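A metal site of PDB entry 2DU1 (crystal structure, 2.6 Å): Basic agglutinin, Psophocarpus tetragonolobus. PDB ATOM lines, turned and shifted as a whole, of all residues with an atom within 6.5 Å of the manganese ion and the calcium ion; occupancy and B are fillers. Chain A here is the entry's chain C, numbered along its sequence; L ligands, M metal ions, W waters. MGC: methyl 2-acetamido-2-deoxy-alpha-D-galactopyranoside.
ND2 of Asn 128 lies within hydrogen-bond range of O3 of the ligand. O3 of the ligand is in hydrogen-bond range of N of Gly 105 (2.8 Å). OD2 of Asp 87 lies within hydrogen-bond range of O3 of the ligand, 2.6 Å away.
OD1 of Asp 131 lies close to NE2 of His 136 (3.2 Å). OD2 of Asp 131 sits close to NE1 of Trp 130. The guanidinium group (NE) of Arg 127 is in hydrogen-bond range of the backbone carbonyl oxygen (O) of Asp 131 (3.2 Å). The backbone carbonyl oxygen (O) of His 136 is in hydrogen-bond range of the backbone NH (N) of Asp 124 (3.0 Å). The side-chain carboxylate of Glu 122 sits close to a ring nitrogen (NE2) of His 136, 2.9 Å away. The backbone carbonyl oxygen (O) of Gly 138 sits at hydrogen-bond distance from the backbone NH (N) of Glu 122 (2.9 Å).
NE2 of His 136 touches the manganese ion, 3.0 Å away. O of Val 144 touches the manganese ion, 3.9 Å away. Along chain A the residues within 4 Å of the manganese ion span positions 122 to 144.
Along chain A the residues within 4 Å of the calcium ion span positions 124 to 131. The nearest printed residue that does not touch the calcium ion is Trp 130 (4.3 Å).
The manganese ion is bound by the side-chain carboxylate (OD1) of Asp 131, water W1, the side-chain carboxylate (OD2) of Asp 124 and the side-chain carboxylate (OE2) of Glu 122. The manganese ion has four donor atoms within binding distance. Slightly farther from the manganese ion lies OE1 of Glu 122 (2.9 Å).
The calcium ion is bound by OD1 of Asn 128 (2.3 Å), OD2 of Asp 131 (2.3 Å), OD2 of Asp 124 (2.4 Å), O of Phe 126 (2.4 Å), water W3 (2.4 Å), water W2 (2.4 Å) and OD1 of Asp 124 (2.6 Å). The calcium ion has seven donor atoms within binding distance.
Water W1 lies within hydrogen-bond range of O of Val 144, OE1 of Glu 122 and NE1 of Trp 130.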
ATOM      1  N   ASP A  87       9.542 -12.513  31.816  1.00  0.00           N
ATOM      2  CA  ASP A  87       9.348 -12.253  30.388  1.00  0.00           C
ATOM      3  C   ASP A  87       7.935 -11.791  30.084  1.00  0.00           C
ATOM      4  O   ASP A  87       7.690 -11.145  29.073  1.00  0.00           O
ATOM      5  CB  ASP A  87       9.633 -13.512  29.573  1.00  0.00           C
ATOM      6  CG  ASP A  87      11.082 -13.604  29.117  1.00  0.00           C
ATOM      7  OD1 ASP A  87      11.932 -14.076  29.909  1.00  0.00           O
ATOM      8  OD2 ASP A  87      11.377 -13.182  27.966  1.00  0.00           O
ATOM      9  N   GLY A 105      11.272 -15.974  26.407  1.00  0.00           N
ATOM     10  CA  GLY A 105      10.370 -15.284  25.506  1.00  0.00           C
ATOM     11  C   GLY A 105       9.269 -16.146  24.916  1.00  0.00           C
ATOM     12  O   GLY A 105       8.390 -15.635  24.229  1.00  0.00           O
ATOM     13  N   PHE A 107       7.260 -17.963  26.800  1.00  0.00           N
ATOM     14  CA  PHE A 107       6.239 -18.037  27.840  1.00  0.00           C
ATOM     15  C   PHE A 107       5.860 -19.434  28.319  1.00  0.00           C
ATOM     16  O   PHE A 107       4.965 -19.579  29.151  1.00  0.00           O
ATOM     17  CB  PHE A 107       4.946 -17.343  27.373  1.00  0.00           C
ATOM     18  CG  PHE A 107       5.167 -15.950  26.849  1.00  0.00           C
ATOM     19  CD1 PHE A 107       5.640 -14.946  27.683  1.00  0.00           C
ATOM     20  CD2 PHE A 107       4.889 -15.650  25.508  1.00  0.00           C
ATOM     21  CE1 PHE A 107       5.852 -13.654  27.195  1.00  0.00           C
ATOM     22  CE2 PHE A 107       5.090 -14.365  25.013  1.00  0.00           C
ATOM     23  CZ  PHE A 107       5.571 -13.367  25.857  1.00  0.00           C
ATOM     24  N   GLU A 122      -0.892 -12.155  24.789  1.00  0.00           N
ATOM     25  CA  GLU A 122       0.278 -11.952  25.624  1.00  0.00           C
ATOM     26  C   GLU A 122       0.431 -10.554  26.203  1.00  0.00           C
ATOM     27  O   GLU A 122      -0.056  -9.573  25.642  1.00  0.00           O
ATOM     28  CB  GLU A 122       1.542 -12.285  24.839  1.00  0.00           C
ATOM     29  CG  GLU A 122       1.777 -11.333  23.675  1.00  0.00           C
ATOM     30  CD  GLU A 122       3.219 -11.300  23.214  1.00  0.00           C
ATOM     31  OE1 GLU A 122       3.801 -12.382  22.989  1.00  0.00           O
ATOM     32  OE2 GLU A 122       3.758 -10.187  23.086  1.00  0.00           O
ATOM     33  N   ASP A 124       3.632  -9.033  27.100  1.00  0.00           N
ATOM     34  CA  ASP A 124       5.078  -9.158  26.990  1.00  0.00           C
ATOM     35  C   ASP A 124       5.829  -8.009  27.636  1.00  0.00           C
ATOM     36  O   ASP A 124       5.572  -6.841  27.358  1.00  0.00           O
ATOM     37  CB  ASP A 124       5.483  -9.298  25.524  1.00  0.00           C
ATOM     38  CG  ASP A 124       6.870  -9.739  25.138  1.00  0.00           C
ATOM     39  OD1 ASP A 124       7.792  -9.611  25.969  1.00  0.00           O
ATOM     40  OD2 ASP A 124       7.040 -10.225  24.011  1.00  0.00           O
ATOM     41  N   THR A 125       6.770  -8.355  28.504  1.00  0.00           N
ATOM     42  CA  THR A 125       7.551  -7.367  29.226  1.00  0.00           C
ATOM     43  C   THR A 125       9.025  -7.302  28.815  1.00  0.00           C
ATOM     44  O   THR A 125       9.738  -6.374  29.209  1.00  0.00           O
ATOM     45  CB  THR A 125       7.453  -7.625  30.743  1.00  0.00           C
ATOM     46  OG1 THR A 125       7.697  -9.014  31.001  1.00  0.00           O
ATOM     47  CG2 THR A 125       6.056  -7.264  31.246  1.00  0.00           C
ATOM     48  N   PHE A 126       9.472  -8.282  28.029  1.00  0.00           N
ATOM     49  CA  PHE A 126      10.855  -8.310  27.569  1.00  0.00           C
ATOM     50  C   PHE A 126      10.907  -8.246  26.057  1.00  0.00           C
ATOM     51  O   PHE A 126      10.206  -8.996  25.368  1.00  0.00           O
ATOM     52  CB  PHE A 126      11.576  -9.578  28.019  1.00  0.00           C
ATOM     53  CG  PHE A 126      13.034  -9.596  27.665  1.00  0.00           C
ATOM     54  CD1 PHE A 126      13.957  -8.886  28.431  1.00  0.00           C
ATOM     55  CD2 PHE A 126      13.489 -10.292  26.549  1.00  0.00           C
ATOM     56  CE1 PHE A 126      15.306  -8.866  28.077  1.00  0.00           C
ATOM     57  CE2 PHE A 126      14.828 -10.278  26.188  1.00  0.00           C
ATOM     58  CZ  PHE A 126      15.745  -9.560  26.954  1.00  0.00           C
ATOM     59  N   ARG A 127      11.775  -7.391  25.522  1.00  0.00           N
ATOM     60  CA  ARG A 127      11.889  -7.255  24.078  1.00  0.00           C
ATOM     61  C   ARG A 127      12.841  -8.249  23.422  1.00  0.00           C
ATOM     62  O   ARG A 127      14.065  -8.080  23.472  1.00  0.00           O
ATOM     63  CB  ARG A 127      12.314  -5.831  23.719  1.00  0.00           C
ATOM     64  CG  ARG A 127      12.342  -5.570  22.218  1.00  0.00           C
ATOM     65  CD  ARG A 127      12.558  -4.103  21.903  1.00  0.00           C
ATOM     66  NE  ARG A 127      12.406  -3.827  20.484  1.00  0.00           N
ATOM     67  CZ  ARG A 127      12.376  -2.605  19.948  1.00  0.00           C
ATOM     68  NH1 ARG A 127      12.489  -1.519  20.702  1.00  0.00           N
ATOM     69  NH2 ARG A 127      12.190  -2.472  18.639  1.00  0.00           N
ATOM     70  N   ASN A 128      12.277  -9.280  22.789  1.00  0.00           N
ATOM     71  CA  ASN A 128      13.073 -10.265  22.086  1.00  0.00           C
ATOM     72  C   ASN A 128      13.379  -9.712  20.688  1.00  0.00           C
ATOM     73  O   ASN A 128      12.855  -8.652  20.322  1.00  0.00           O
ATOM     74  CB  ASN A 128      12.317 -11.592  21.951  1.00  0.00           C
ATOM     75  CG  ASN A 128      12.172 -12.314  23.282  1.00  0.00           C
ATOM     76  OD1 ASN A 128      11.329 -11.964  24.110  1.00  0.00           O
ATOM     77  ND2 ASN A 128      12.997 -13.334  23.478  1.00  0.00           N
ATOM     78  N   TRP A 130      12.282 -10.494  17.973  1.00  0.00           N
ATOM     79  CA  TRP A 130      11.053 -10.427  17.189  1.00  0.00           C
ATOM     80  C   TRP A 130       9.995  -9.486  17.753  1.00  0.00           C
ATOM     81  O   TRP A 130       8.881  -9.411  17.230  1.00  0.00           O
ATOM     82  CB  TRP A 130      10.461 -11.840  17.089  1.00  0.00           C
ATOM     83  CG  TRP A 130      10.220 -12.458  18.439  1.00  0.00           C
ATOM     84  CD1 TRP A 130       9.259 -12.101  19.335  1.00  0.00           C
ATOM     85  CD2 TRP A 130      10.967 -13.512  19.052  1.00  0.00           C
ATOM     86  NE1 TRP A 130       9.365 -12.873  20.467  1.00  0.00           N
ATOM     87  CE2 TRP A 130      10.405 -13.751  20.314  1.00  0.00           C
ATOM     88  CE3 TRP A 130      12.068 -14.287  18.642  1.00  0.00           C
ATOM     89  CZ2 TRP A 130      10.890 -14.727  21.186  1.00  0.00           C
ATOM     90  CZ3 TRP A 130      12.551 -15.265  19.505  1.00  0.00           C
ATOM     91  CH2 TRP A 130      11.965 -15.483  20.770  1.00  0.00           C
ATOM     92  N   ASP A 131      10.344  -8.766  18.820  1.00  0.00           N
ATOM     93  CA  ASP A 131       9.388  -7.881  19.480  1.00  0.00           C
ATOM     94  C   ASP A 131       9.553  -6.399  19.227  1.00  0.00           C
ATOM     95  O   ASP A 131      10.636  -5.921  18.918  1.00  0.00           O
ATOM     96  CB  ASP A 131       9.469  -8.049  21.006  1.00  0.00           C
ATOM     97  CG  ASP A 131       8.789  -9.294  21.506  1.00  0.00           C
ATOM     98  OD1 ASP A 131       7.569  -9.434  21.296  1.00  0.00           O
ATOM     99  OD2 ASP A 131       9.467 -10.131  22.106  1.00  0.00           O
ATOM    100  N   PRO A 132       8.431  -5.666  19.336  1.00  0.00           N
ATOM    101  CA  PRO A 132       8.403  -4.213  19.154  1.00  0.00           C
ATOM    102  C   PRO A 132       8.674  -3.728  20.580  1.00  0.00           C
ATOM    103  O   PRO A 132       8.899  -4.550  21.483  1.00  0.00           O
ATOM    104  CB  PRO A 132       6.957  -3.948  18.737  1.00  0.00           C
ATOM    105  CG  PRO A 132       6.194  -5.012  19.451  1.00  0.00           C
ATOM    106  CD  PRO A 132       7.062  -6.223  19.247  1.00  0.00           C
ATOM    107  N   ILE A 134       8.477  -2.722  24.422  1.00  0.00           N
ATOM    108  CA  ILE A 134       7.684  -3.327  25.498  1.00  0.00           C
ATOM    109  C   ILE A 134       7.447  -2.279  26.578  1.00  0.00           C
ATOM    110  O   ILE A 134       8.111  -1.257  26.619  1.00  0.00           O
ATOM    111  CB  ILE A 134       8.394  -4.559  26.101  1.00  0.00           C
ATOM    112  CG1 ILE A 134       9.846  -4.228  26.459  1.00  0.00           C
ATOM    113  CG2 ILE A 134       8.354  -5.688  25.107  1.00  0.00           C
ATOM    114  CD1 ILE A 134      10.030  -3.415  27.770  1.00  0.00           C
ATOM    115  N   HIS A 136       3.959  -4.661  25.903  1.00  0.00           N
ATOM    116  CA  HIS A 136       2.938  -4.587  24.862  1.00  0.00           C
ATOM    117  C   HIS A 136       1.994  -5.754  24.958  1.00  0.00           C
ATOM    118  O   HIS A 136       2.327  -6.786  25.552  1.00  0.00           O
ATOM    119  CB  HIS A 136       3.588  -4.516  23.465  1.00  0.00           C
ATOM    120  CG  HIS A 136       4.411  -5.716  23.105  1.00  0.00           C
ATOM    121  ND1 HIS A 136       5.780  -5.663  22.918  1.00  0.00           N
ATOM    122  CD2 HIS A 136       4.050  -7.004  22.861  1.00  0.00           C
ATOM    123  CE1 HIS A 136       6.222  -6.855  22.575  1.00  0.00           C
ATOM    124  NE2 HIS A 136       5.196  -7.693  22.534  1.00  0.00           N
ATOM    125  N   GLY A 138      -0.160  -8.470  22.798  1.00  0.00           N
ATOM    126  CA  GLY A 138      -0.036  -9.027  21.464  1.00  0.00           C
ATOM    127  C   GLY A 138      -0.983 -10.190  21.291  1.00  0.00           C
ATOM    128  O   GLY A 138      -1.330 -10.878  22.250  1.00  0.00           O
ATOM    129  N   ASP A 140      -1.274 -13.689  19.547  1.00  0.00           N
ATOM    130  CA  ASP A 140      -0.446 -14.715  18.935  1.00  0.00           C
ATOM    131  C   ASP A 140      -1.212 -15.923  18.435  1.00  0.00           C
ATOM    132  O   ASP A 140      -2.033 -16.492  19.149  1.00  0.00           O
ATOM    133  CB  ASP A 140       0.591 -15.239  19.938  1.00  0.00           C
ATOM    134  CG  ASP A 140       1.279 -14.121  20.706  1.00  0.00           C
ATOM    135  OD1 ASP A 140       1.431 -13.008  20.142  1.00  0.00           O
ATOM    136  OD2 ASP A 140       1.679 -14.376  21.867  1.00  0.00           O
ATOM    137  N   VAL A 144       4.870 -16.792  18.689  1.00  0.00           N
ATOM    138  CA  VAL A 144       4.980 -15.712  19.651  1.00  0.00           C
ATOM    139  C   VAL A 144       5.307 -14.437  18.879  1.00  0.00           C
ATOM    140  O   VAL A 144       5.619 -13.399  19.467  1.00  0.00           O
ATOM    141  CB  VAL A 144       6.063 -16.019  20.729  1.00  0.00           C
ATOM    142  CG1 VAL A 144       7.414 -15.429  20.331  1.00  0.00           C
ATOM    143  CG2 VAL A 144       5.622 -15.484  22.069  1.00  0.00           C
ATOM    144  N   ILE A 145       5.258 -14.524  17.555  1.00  0.00           N
ATOM    145  CA  ILE A 145       5.489 -13.355  16.695  1.00  0.00           C
ATOM    146  C   ILE A 145       4.075 -12.859  16.417  1.00  0.00           C
ATOM    147  O   ILE A 145       3.424 -13.252  15.442  1.00  0.00           O
ATOM    148  CB  ILE A 145       6.162 -13.731  15.362  1.00  0.00           C
ATOM    149  CG1 ILE A 145       7.511 -14.411  15.648  1.00  0.00           C
ATOM    150  CG2 ILE A 145       6.392 -12.469  14.532  1.00  0.00           C
ATOM    151  CD1 ILE A 145       8.294 -14.790  14.382  1.00  0.00           C
ATOM    152  N   SER A 146       3.589 -12.013  17.314  1.00  0.00           N
ATOM    153  CA  SER A 146       2.228 -11.465  17.265  1.00  0.00           C
ATOM    154  C   SER A 146       1.758 -10.966  15.913  1.00  0.00           C
ATOM    155  O   SER A 146       2.525 -10.359  15.144  1.00  0.00           O
ATOM    156  CB  SER A 146       2.087 -10.344  18.292  1.00  0.00           C
ATOM    157  OG  SER A 146       2.601 -10.753  19.539  1.00  0.00           O
ATOM    158  N   THR A 149      -0.053  -5.970  17.723  1.00  0.00           N
ATOM    159  CA  THR A 149       0.561  -5.535  18.971  1.00  0.00           C
ATOM    160  C   THR A 149       0.172  -4.109  19.334  1.00  0.00           C
ATOM    161  O   THR A 149      -0.084  -3.282  18.458  1.00  0.00           O
ATOM    162  CB  THR A 149       2.097  -5.614  18.813  1.00  0.00           C
ATOM    163  OG1 THR A 149       2.549  -6.933  19.168  1.00  0.00           O
ATOM    164  CG2 THR A 149       2.794  -4.599  19.635  1.00  0.00           C
HETATM  165  O6  MGC L   1      17.959 -12.008  30.052  1.00  0.00           O
HETATM  166  C6  MGC L   1      16.602 -12.414  29.920  1.00  0.00           C
HETATM  167  C5  MGC L   1      16.312 -12.841  28.511  1.00  0.00           C
HETATM  168  O5  MGC L   1      17.217 -13.943  28.180  1.00  0.00           O
HETATM  169  C1  MGC L   1      17.095 -14.430  26.791  1.00  0.00           C
HETATM  170  O1  MGC L   1      17.542 -13.489  25.806  1.00  0.00           O
HETATM  171  CM  MGC L   1      18.886 -12.985  25.940  1.00  0.00           C
HETATM  172  C2  MGC L   1      15.645 -14.880  26.510  1.00  0.00           C
HETATM  173  N2  MGC L   1      15.513 -15.314  25.117  1.00  0.00           N
HETATM  174  C7  MGC L   1      14.785 -16.382  24.745  1.00  0.00           C
HETATM  175  O7  MGC L   1      14.162 -17.111  25.527  1.00  0.00           O
HETATM  176  C8  MGC L   1      14.775 -16.678  23.242  1.00  0.00           C
HETATM  177  C3  MGC L   1      14.663 -13.720  26.831  1.00  0.00           C
HETATM  178  O3  MGC L   1      13.321 -14.126  26.591  1.00  0.00           O
HETATM  179  C4  MGC L   1      14.843 -13.281  28.306  1.00  0.00           C
HETATM  180  O4  MGC L   1      14.520 -14.354  29.185  1.00  0.00           O
HETATM  181 MN    MN M   1       5.813 -10.548  22.107  1.00  0.00          MN
HETATM  182 CA    CA M   2       9.291 -10.901  24.279  1.00  0.00          CA
HETATM  183  O   HOH W   1       6.383 -12.751  21.875  1.00  0.00           O
HETATM  184  O   HOH W   2       9.171 -11.838  26.522  1.00  0.00           O
HETATM  185  O   HOH W   3       8.167 -12.987  23.823  1.00  0.00           O
